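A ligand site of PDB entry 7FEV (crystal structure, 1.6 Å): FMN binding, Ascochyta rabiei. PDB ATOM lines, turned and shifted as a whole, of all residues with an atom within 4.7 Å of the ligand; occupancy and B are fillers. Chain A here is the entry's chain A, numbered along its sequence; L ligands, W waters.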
ATOM      1  N   GLY A  37      22.293 -14.209   3.478  1.00  0.00           N
ATOM      2  CA  GLY A  37      21.547 -13.459   4.467  1.00  0.00           C
ATOM      3  C   GLY A  37      22.180 -13.533   5.833  1.00  0.00           C
ATOM      4  O   GLY A  37      22.804 -14.522   6.208  1.00  0.00           O
ATOM      5  N   ALA A  38      22.039 -12.438   6.577  1.00  0.00           N
ATOM      6  CA  ALA A  38      22.549 -12.370   7.942  1.00  0.00           C
ATOM      7  C   ALA A  38      21.956 -13.506   8.777  1.00  0.00           C
ATOM      8  O   ALA A  38      20.751 -13.758   8.719  1.00  0.00           O
ATOM      9  CB  ALA A  38      22.164 -11.039   8.571  1.00  0.00           C
ATOM     10  N   MET A  39      22.803 -14.167   9.564  1.00  0.00           N
ATOM     11  CA  MET A  39      22.314 -15.186  10.502  1.00  0.00           C
ATOM     12  C   MET A  39      23.090 -15.068  11.799  1.00  0.00           C
ATOM     13  O   MET A  39      24.311 -15.287  11.817  1.00  0.00           O
ATOM     14  CB  MET A  39      22.412 -16.600   9.927  1.00  0.00           C
ATOM     15  CG  MET A  39      21.342 -16.878   8.858  1.00  0.00           C
ATOM     16  SD  MET A  39      21.428 -18.550   8.147  1.00  0.00           S
ATOM     17  CE  MET A  39      22.944 -18.432   7.211  1.00  0.00           C
ATOM     18  N   THR A  40      22.373 -14.767  12.885  1.00  0.00           N
ATOM     19  CA  THR A  40      23.000 -14.688  14.209  1.00  0.00           C
ATOM     20  C   THR A  40      23.657 -16.033  14.545  1.00  0.00           C
ATOM     21  O   THR A  40      23.000 -17.078  14.532  1.00  0.00           O
ATOM     22  CB  THR A  40      21.932 -14.265  15.247  1.00  0.00           C
ATOM     23  OG1 THR A  40      22.497 -14.219  16.565  1.00  0.00           O
ATOM     24  CG2 THR A  40      20.679 -15.174  15.247  1.00  0.00           C
ATOM     25  N   GLY A  79      25.803 -12.121  10.792  1.00  0.00           N
ATOM     26  CA  GLY A  79      24.672 -11.982  11.691  1.00  0.00           C
ATOM     27  C   GLY A  79      24.751 -10.655  12.429  1.00  0.00           C
ATOM     28  O   GLY A  79      25.785  -9.975  12.425  1.00  0.00           O
ATOM     29  N   ASN A  80      23.649 -10.262  13.081  1.00  0.00           N
ATOM     30  CA  ASN A  80      23.609  -8.930  13.674  1.00  0.00           C
ATOM     31  C   ASN A  80      24.699  -8.755  14.728  1.00  0.00           C
ATOM     32  O   ASN A  80      24.979  -9.648  15.527  1.00  0.00           O
ATOM     33  CB  ASN A  80      22.214  -8.560  14.229  1.00  0.00           C
ATOM     34  CG  ASN A  80      21.707  -9.428  15.401  1.00  0.00           C
ATOM     35  OD1 ASN A  80      22.536  -9.849  16.221  1.00  0.00           O
ATOM     36  ND2 ASN A  80      20.418  -9.727  15.480  1.00  0.00           N
ATOM     37  N   GLN A 127      26.353  -6.604   9.537  1.00  0.00           N
ATOM     38  CA  GLN A 127      25.027  -6.158   9.923  1.00  0.00           C
ATOM     39  C   GLN A 127      25.090  -5.688  11.354  1.00  0.00           C
ATOM     40  O   GLN A 127      25.636  -6.379  12.214  1.00  0.00           O
ATOM     41  CB  GLN A 127      23.988  -7.272   9.803  1.00  0.00           C
ATOM     42  CG  GLN A 127      22.579  -6.707  10.012  1.00  0.00           C
ATOM     43  CD  GLN A 127      21.514  -7.767  10.154  1.00  0.00           C
ATOM     44  OE1 GLN A 127      21.479  -8.517  11.140  1.00  0.00           O
ATOM     45  NE2 GLN A 127      20.618  -7.834   9.175  1.00  0.00           N
ATOM     46  N   HIS A 196      20.186  -3.050  10.488  1.00  0.00           N
ATOM     47  CA  HIS A 196      19.110  -4.015  10.685  1.00  0.00           C
ATOM     48  C   HIS A 196      17.830  -3.248  10.956  1.00  0.00           C
ATOM     49  O   HIS A 196      17.564  -2.823  12.089  1.00  0.00           O
ATOM     50  CB  HIS A 196      19.431  -4.985  11.821  1.00  0.00           C
ATOM     51  CG  HIS A 196      18.540  -6.178  11.866  1.00  0.00           C
ATOM     52  ND1 HIS A 196      17.333  -6.238  11.195  1.00  0.00           N
ATOM     53  CD2 HIS A 196      18.676  -7.376  12.501  1.00  0.00           C
ATOM     54  CE1 HIS A 196      16.768  -7.416  11.420  1.00  0.00           C
ATOM     55  NE2 HIS A 196      17.567  -8.126  12.197  1.00  0.00           N
ATOM     56  N   LYS A 249      18.291  -3.641   5.790  1.00  0.00           N
ATOM     57  CA  LYS A 249      17.318  -4.712   5.679  1.00  0.00           C
ATOM     58  C   LYS A 249      15.961  -4.212   6.157  1.00  0.00           C
ATOM     59  O   LYS A 249      15.855  -3.675   7.269  1.00  0.00           O
ATOM     60  CB  LYS A 249      17.760  -5.924   6.494  1.00  0.00           C
ATOM     61  CG  LYS A 249      16.843  -7.139   6.272  1.00  0.00           C
ATOM     62  CD  LYS A 249      17.414  -8.360   6.944  1.00  0.00           C
ATOM     63  CE  LYS A 249      16.745  -9.618   6.417  1.00  0.00           C
ATOM     64  NZ  LYS A 249      17.436 -10.836   6.918  1.00  0.00           N
ATOM     65  N   SER A 283      12.599  -8.303   2.919  1.00  0.00           N
ATOM     66  CA  SER A 283      12.222  -9.591   3.503  1.00  0.00           C
ATOM     67  C   SER A 283      10.796  -9.509   4.017  1.00  0.00           C
ATOM     68  O   SER A 283      10.164  -8.455   4.005  1.00  0.00           O
ATOM     69  CB  SER A 283      13.169  -9.974   4.644  1.00  0.00           C
ATOM     70  OG  SER A 283      13.221  -8.921   5.591  1.00  0.00           O
ATOM     71  N   THR A 325      15.221 -11.542   0.086  1.00  0.00           N
ATOM     72  CA  THR A 325      15.675 -12.680   0.874  1.00  0.00           C
ATOM     73  C   THR A 325      14.471 -13.368   1.481  1.00  0.00           C
ATOM     74  O   THR A 325      13.683 -12.718   2.185  1.00  0.00           O
ATOM     75  CB  THR A 325      16.620 -12.238   2.003  1.00  0.00           C
ATOM     76  OG1 THR A 325      17.735 -11.510   1.457  1.00  0.00           O
ATOM     77  CG2 THR A 325      17.151 -13.462   2.745  1.00  0.00           C
ATOM     78  N   GLY A 326      14.344 -14.668   1.238  1.00  0.00           N
ATOM     79  CA  GLY A 326      13.284 -15.432   1.860  1.00  0.00           C
ATOM     80  C   GLY A 326      12.717 -16.488   0.924  1.00  0.00           C
ATOM     81  O   GLY A 326      12.059 -16.169  -0.068  1.00  0.00           O
ATOM     82  N   GLY A 327      13.034 -17.740   1.224  1.00  0.00           N
ATOM     83  CA  GLY A 327      12.411 -18.873   0.565  1.00  0.00           C
ATOM     84  C   GLY A 327      13.036 -19.340  -0.737  1.00  0.00           C
ATOM     85  O   GLY A 327      12.535 -20.295  -1.322  1.00  0.00           O
ATOM     86  N   PHE A 328      14.100 -18.711  -1.215  1.00  0.00           N
ATOM     87  CA  PHE A 328      14.691 -19.158  -2.480  1.00  0.00           C
ATOM     88  C   PHE A 328      15.358 -20.514  -2.329  1.00  0.00           C
ATOM     89  O   PHE A 328      16.162 -20.728  -1.416  1.00  0.00           O
ATOM     90  CB  PHE A 328      15.709 -18.142  -2.994  1.00  0.00           C
ATOM     91  CG  PHE A 328      15.082 -16.933  -3.642  1.00  0.00           C
ATOM     92  CD1 PHE A 328      14.330 -17.060  -4.791  1.00  0.00           C
ATOM     93  CD2 PHE A 328      15.280 -15.672  -3.099  1.00  0.00           C
ATOM     94  CE1 PHE A 328      13.756 -15.953  -5.398  1.00  0.00           C
ATOM     95  CE2 PHE A 328      14.701 -14.549  -3.710  1.00  0.00           C
ATOM     96  CZ  PHE A 328      13.942 -14.701  -4.848  1.00  0.00           C
ATOM     97  N   GLY A 345      18.810 -13.133  -2.004  1.00  0.00           N
ATOM     98  CA  GLY A 345      19.424 -13.487  -0.740  1.00  0.00           C
ATOM     99  C   GLY A 345      18.978 -14.874  -0.336  1.00  0.00           C
ATOM    100  O   GLY A 345      17.818 -15.236  -0.526  1.00  0.00           O
ATOM    101  N   LEU A 346      19.929 -15.645   0.208  1.00  0.00           N
ATOM    102  CA  LEU A 346      19.712 -16.982   0.722  1.00  0.00           C
ATOM    103  C   LEU A 346      20.315 -17.054   2.108  1.00  0.00           C
ATOM    104  O   LEU A 346      21.453 -16.632   2.307  1.00  0.00           O
ATOM    105  CB  LEU A 346      20.360 -18.050  -0.176  1.00  0.00           C
ATOM    106  CG  LEU A 346      19.606 -18.299  -1.475  1.00  0.00           C
ATOM    107  CD1 LEU A 346      20.145 -17.404  -2.571  1.00  0.00           C
ATOM    108  CD2 LEU A 346      19.718 -19.760  -1.853  1.00  0.00           C
ATOM    109  N   ALA A 347      19.550 -17.587   3.070  1.00  0.00           N
ATOM    110  CA  ALA A 347      20.067 -17.760   4.413  1.00  0.00           C
ATOM    111  C   ALA A 347      20.103 -19.243   4.767  1.00  0.00           C
ATOM    112  O   ALA A 347      21.182 -19.840   4.723  1.00  0.00           O
ATOM    113  CB  ALA A 347      19.231 -16.968   5.431  1.00  0.00           C
ATOM    114  N   ARG A 348      18.944 -19.824   5.085  1.00  0.00           N
ATOM    115  CA  ARG A 348      18.936 -21.222   5.520  1.00  0.00           C
ATOM    116  C   ARG A 348      19.599 -22.166   4.519  1.00  0.00           C
ATOM    117  O   ARG A 348      20.328 -23.062   4.968  1.00  0.00           O
ATOM    118  CB  ARG A 348      17.489 -21.648   5.828  1.00  0.00           C
ATOM    119  CG  ARG A 348      16.982 -21.044   7.167  1.00  0.00           C
ATOM    120  CD  ARG A 348      15.494 -21.253   7.326  1.00  0.00           C
ATOM    121  NE  ARG A 348      14.742 -20.592   6.257  1.00  0.00           N
ATOM    122  CZ  ARG A 348      13.434 -20.725   6.064  1.00  0.00           C
ATOM    123  NH1 ARG A 348      12.701 -21.473   6.888  1.00  0.00           N
ATOM    124  NH2 ARG A 348      12.844 -20.091   5.041  1.00  0.00           N
ATOM    125  N   PRO A 349      19.432 -22.015   3.196  1.00  0.00           N
ATOM    126  CA  PRO A 349      20.139 -22.929   2.284  1.00  0.00           C
ATOM    127  C   PRO A 349      21.647 -22.816   2.358  1.00  0.00           C
ATOM    128  O   PRO A 349      22.329 -23.811   2.054  1.00  0.00           O
ATOM    129  CB  PRO A 349      19.610 -22.526   0.906  1.00  0.00           C
ATOM    130  CG  PRO A 349      18.247 -21.988   1.173  1.00  0.00           C
ATOM    131  CD  PRO A 349      18.435 -21.205   2.471  1.00  0.00           C
ATOM    132  N   THR A 381      13.421 -24.925  11.618  1.00  0.00           N
ATOM    133  CA  THR A 381      14.353 -24.584  10.546  1.00  0.00           C
ATOM    134  C   THR A 381      15.420 -23.620  11.030  1.00  0.00           C
ATOM    135  O   THR A 381      16.555 -23.661  10.540  1.00  0.00           O
ATOM    136  CB  THR A 381      13.648 -23.990   9.318  1.00  0.00           C
ATOM    137  OG1 THR A 381      13.066 -22.717   9.656  1.00  0.00           O
ATOM    138  CG2 THR A 381      12.594 -24.932   8.737  1.00  0.00           C
ATOM    139  N   ASN A 382      15.091 -22.742  11.970  1.00  0.00           N
ATOM    140  CA  ASN A 382      16.098 -21.839  12.490  1.00  0.00           C
ATOM    141  C   ASN A 382      17.111 -22.583  13.347  1.00  0.00           C
ATOM    142  O   ASN A 382      18.318 -22.368  13.211  1.00  0.00           O
ATOM    143  CB  ASN A 382      15.437 -20.701  13.274  1.00  0.00           C
ATOM    144  CG  ASN A 382      14.783 -19.684  12.362  1.00  0.00           C
ATOM    145  OD1 ASN A 382      14.418 -18.596  12.789  1.00  0.00           O
ATOM    146  ND2 ASN A 382      14.577 -20.062  11.102  1.00  0.00           N
ATOM    147  N   ALA A 385      19.504 -24.377  11.005  1.00  0.00           N
ATOM    148  CA  ALA A 385      20.514 -23.536  10.374  1.00  0.00           C
ATOM    149  C   ALA A 385      21.608 -23.141  11.349  1.00  0.00           C
ATOM    150  O   ALA A 385      22.785 -23.163  11.007  1.00  0.00           O
ATOM    151  CB  ALA A 385      19.862 -22.282   9.772  1.00  0.00           C
ATOM    152  N   GLY A 386      21.222 -22.771  12.581  1.00  0.00           N
ATOM    153  CA  GLY A 386      22.235 -22.433  13.571  1.00  0.00           C
ATOM    154  C   GLY A 386      23.144 -23.611  13.900  1.00  0.00           C
ATOM    155  O   GLY A 386      24.358 -23.442  14.078  1.00  0.00           O
ATOM    156  N   MET A 389      25.750 -23.928  11.179  1.00  0.00           N
ATOM    157  CA  MET A 389      26.806 -22.930  11.322  1.00  0.00           C
ATOM    158  C   MET A 389      27.799 -23.362  12.407  1.00  0.00           C
ATOM    159  O   MET A 389      29.011 -23.194  12.243  1.00  0.00           O
ATOM    160  CB  MET A 389      26.225 -21.554  11.654  1.00  0.00           C
ATOM    161  CG  MET A 389      25.466 -20.909  10.515  1.00  0.00           C
ATOM    162  SD  MET A 389      25.003 -19.205  10.942  1.00  0.00           S
ATOM    163  CE  MET A 389      23.659 -19.497  12.095  1.00  0.00           C
ATOM    164  N   TYR A 432      24.009 -22.670  19.592  1.00  0.00           N
ATOM    165  CA  TYR A 432      23.059 -23.619  19.027  1.00  0.00           C
ATOM    166  C   TYR A 432      23.419 -25.045  19.449  1.00  0.00           C
ATOM    167  O   TYR A 432      24.279 -25.274  20.297  1.00  0.00           O
ATOM    168  CB  TYR A 432      23.050 -23.477  17.500  1.00  0.00           C
ATOM    169  CG  TYR A 432      22.463 -22.163  17.010  1.00  0.00           C
ATOM    170  CD1 TYR A 432      21.098 -21.959  16.954  1.00  0.00           C
ATOM    171  CD2 TYR A 432      23.309 -21.134  16.583  1.00  0.00           C
ATOM    172  CE1 TYR A 432      20.574 -20.743  16.487  1.00  0.00           C
ATOM    173  CE2 TYR A 432      22.792 -19.933  16.122  1.00  0.00           C
ATOM    174  CZ  TYR A 432      21.435 -19.739  16.085  1.00  0.00           C
ATOM    175  OH  TYR A 432      20.931 -18.559  15.606  1.00  0.00           O
HETATM  176  N1  LIG L   1      18.127 -11.883   9.740  1.00  0.00           N
HETATM  177  C1  LIG L   1      18.748 -10.732  10.149  1.00  0.00           C
HETATM  178  O1  LIG L   1      18.431  -9.685   9.595  1.00  0.00           O
HETATM  179  N2  LIG L   1      19.702 -10.744  11.137  1.00  0.00           N
HETATM  180  C2  LIG L   1      20.057 -11.915  11.777  1.00  0.00           C
HETATM  181  O2  LIG L   1      20.951 -11.904  12.640  1.00  0.00           O
HETATM  182  C3  LIG L   1      19.448 -13.093  11.338  1.00  0.00           C
HETATM  183  N3  LIG L   1      19.761 -14.293  11.943  1.00  0.00           N
HETATM  184  C4  LIG L   1      19.206 -15.464  11.500  1.00  0.00           C
HETATM  185  C5  LIG L   1      19.609 -16.646  12.098  1.00  0.00           C
HETATM  186  C6  LIG L   1      19.037 -17.842  11.676  1.00  0.00           C
HETATM  187  C7  LIG L   1      19.457 -19.137  12.320  1.00  0.00           C
HETATM  188  C8  LIG L   1      18.084 -17.820  10.661  1.00  0.00           C
HETATM  189  C9  LIG L   1      17.456 -19.086  10.177  1.00  0.00           C
HETATM  190  C10 LIG L   1      17.686 -16.626  10.057  1.00  0.00           C
HETATM  191  C11 LIG L   1      18.248 -15.427  10.479  1.00  0.00           C
HETATM  192  N4  LIG L   1      17.874 -14.224   9.891  1.00  0.00           N
HETATM  193  C12 LIG L   1      18.486 -13.068  10.323  1.00  0.00           C
HETATM  194  C13 LIG L   1      16.882 -14.120   8.784  1.00  0.00           C
HETATM  195  C14 LIG L   1      17.576 -14.466   7.457  1.00  0.00           C
HETATM  196  O3  LIG L   1      18.560 -13.507   7.123  1.00  0.00           O
HETATM  197  C15 LIG L   1      16.576 -14.544   6.306  1.00  0.00           C
HETATM  198  O4  LIG L   1      15.912 -13.314   6.185  1.00  0.00           O
HETATM  199  C16 LIG L   1      15.499 -15.616   6.518  1.00  0.00           C
HETATM  200  O5  LIG L   1      16.097 -16.773   7.087  1.00  0.00           O
HETATM  201  C17 LIG L   1      14.764 -15.936   5.216  1.00  0.00           C
HETATM  202  O6  LIG L   1      15.690 -16.316   4.214  1.00  0.00           O
HETATM  203  P1  LIG L   1      15.804 -17.896   3.794  1.00  0.00           P
HETATM  204  O7  LIG L   1      16.414 -18.589   5.010  1.00  0.00           O
HETATM  205  O8  LIG L   1      14.443 -18.409   3.438  1.00  0.00           O
HETATM  206  O9  LIG L   1      16.793 -17.926   2.646  1.00  0.00           O
HETATM  207  O   HOH W   1      16.895 -10.950  12.855  1.00  0.00           O
HETATM  208  O   HOH W   2      20.002 -10.574   5.872  1.00  0.00           O
HETATM  209  O   HOH W   3      15.350 -20.419   1.359  1.00  0.00           O
HETATM  210  O   HOH W   4      15.902 -16.937   0.321  1.00  0.00           O
HETATM  211  O   HOH W   5      13.484 -12.733   7.428  1.00  0.00           O
HETATM  212  O   HOH W   6      14.026 -17.781   8.916  1.00  0.00           O
HETATM  213  O   HOH W   7      18.536 -11.618  14.812  1.00  0.00           O
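Merely in contact with the ligand: Gly 37 (3.8 Å), Met 39 (3.1 Å), Gly 79 (3.8 Å), Thr 325 (3.5 Å), Gly 326 (3.5 Å), Leu 346 (3.6 Å), Pro 349 (3.7 Å), Asn 382 (3.2 Å) and Tyr 432 (3.6 Å).
Within 4 Å of the ligand: Gly 37, Ala 38, Met 39, Thr 40, Gly 79, Asn 80, Gln 127, His 196, Lys 249, Thr 325, Gly 326, Gly 327, Leu 346, Ala 347, Arg 348, Pro 349, Asn 382 and Tyr 432.
Water W6 lies within hydrogen-bond range of O5 of the ligand and ND2 of Asn 382.
Water W3 lies within hydrogen-bond range of O of Phe 328 (2.9 Å) and O8 of the ligand (3.0 Å).
Water W7 lies within hydrogen-bond range of ND2 of Asn 80 (2.8 Å) and O2 of the ligand (3.3 Å).
Water W1 lies within hydrogen-bond range of NE2 of His 196 and N2 of the ligand.
Water W2 lies within hydrogen-bond range of NZ of Lys 249 (2.8 Å), N of Ala 38 (2.8 Å) and O3 of the ligand (3.5 Å).
N of Gly 327 is in hydrogen-bond range of O8 of the ligand, at 2.7 Å.
The backbone carbonyl oxygen (O) of Ala 38 is in hydrogen-bond range of an oxygen (O3) of the ligand, at 2.7 Å.
The backbone NH (N) of Ala 347 lies within hydrogen-bond range of an oxygen (O9) of the ligand.
The backbone NH (N) of Arg 348 lies within hydrogen-bond range of an oxygen (O7) of the ligand, at 2.8 Å.
NH2 of Arg 348 lies within salt-bridge range of O8 of the ligand (2.8 Å).
The backbone NH (N) of Thr 40 lies within hydrogen-bond range of a nitrogen (N3) of the ligand (2.8 Å).
A nitrogen (N2) of the ligand lies within hydrogen-bond range of the side-chain amide oxygen of Gln 127.
An oxygen (O3) of the ligand is in hydrogen-bond range of the side-chain amino group (NZ) of Lys 249.
An oxygen (O1) of the ligand lies within hydrogen-bond range of a ring nitrogen (NE2) of His 196, at 3.2 Å.
The backbone NH of Asn 80 sits at hydrogen-bond distance from an oxygen (O2) of the ligand (3.2 Å).
OG1 of Thr 381 lies within hydrogen-bond range of NH1 of Arg 348 (3.1 Å).
The backbone carbonyl oxygen (O) of Thr 40 lies within hydrogen-bond range of the side-chain hydroxyl (OH) of Tyr 432, at 2.8 Å.
OE1 of Gln 127 lies close to N of Asn 80 (3.4 Å).
The side-chain amide nitrogen (ND2) of Asn 382 is in hydrogen-bond range of the side-chain hydroxyl (OG1) of Thr 381 (3.4 Å).
N of Gly 37 lies within hydrogen-bond range of O of Leu 346 (2.8 Å).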
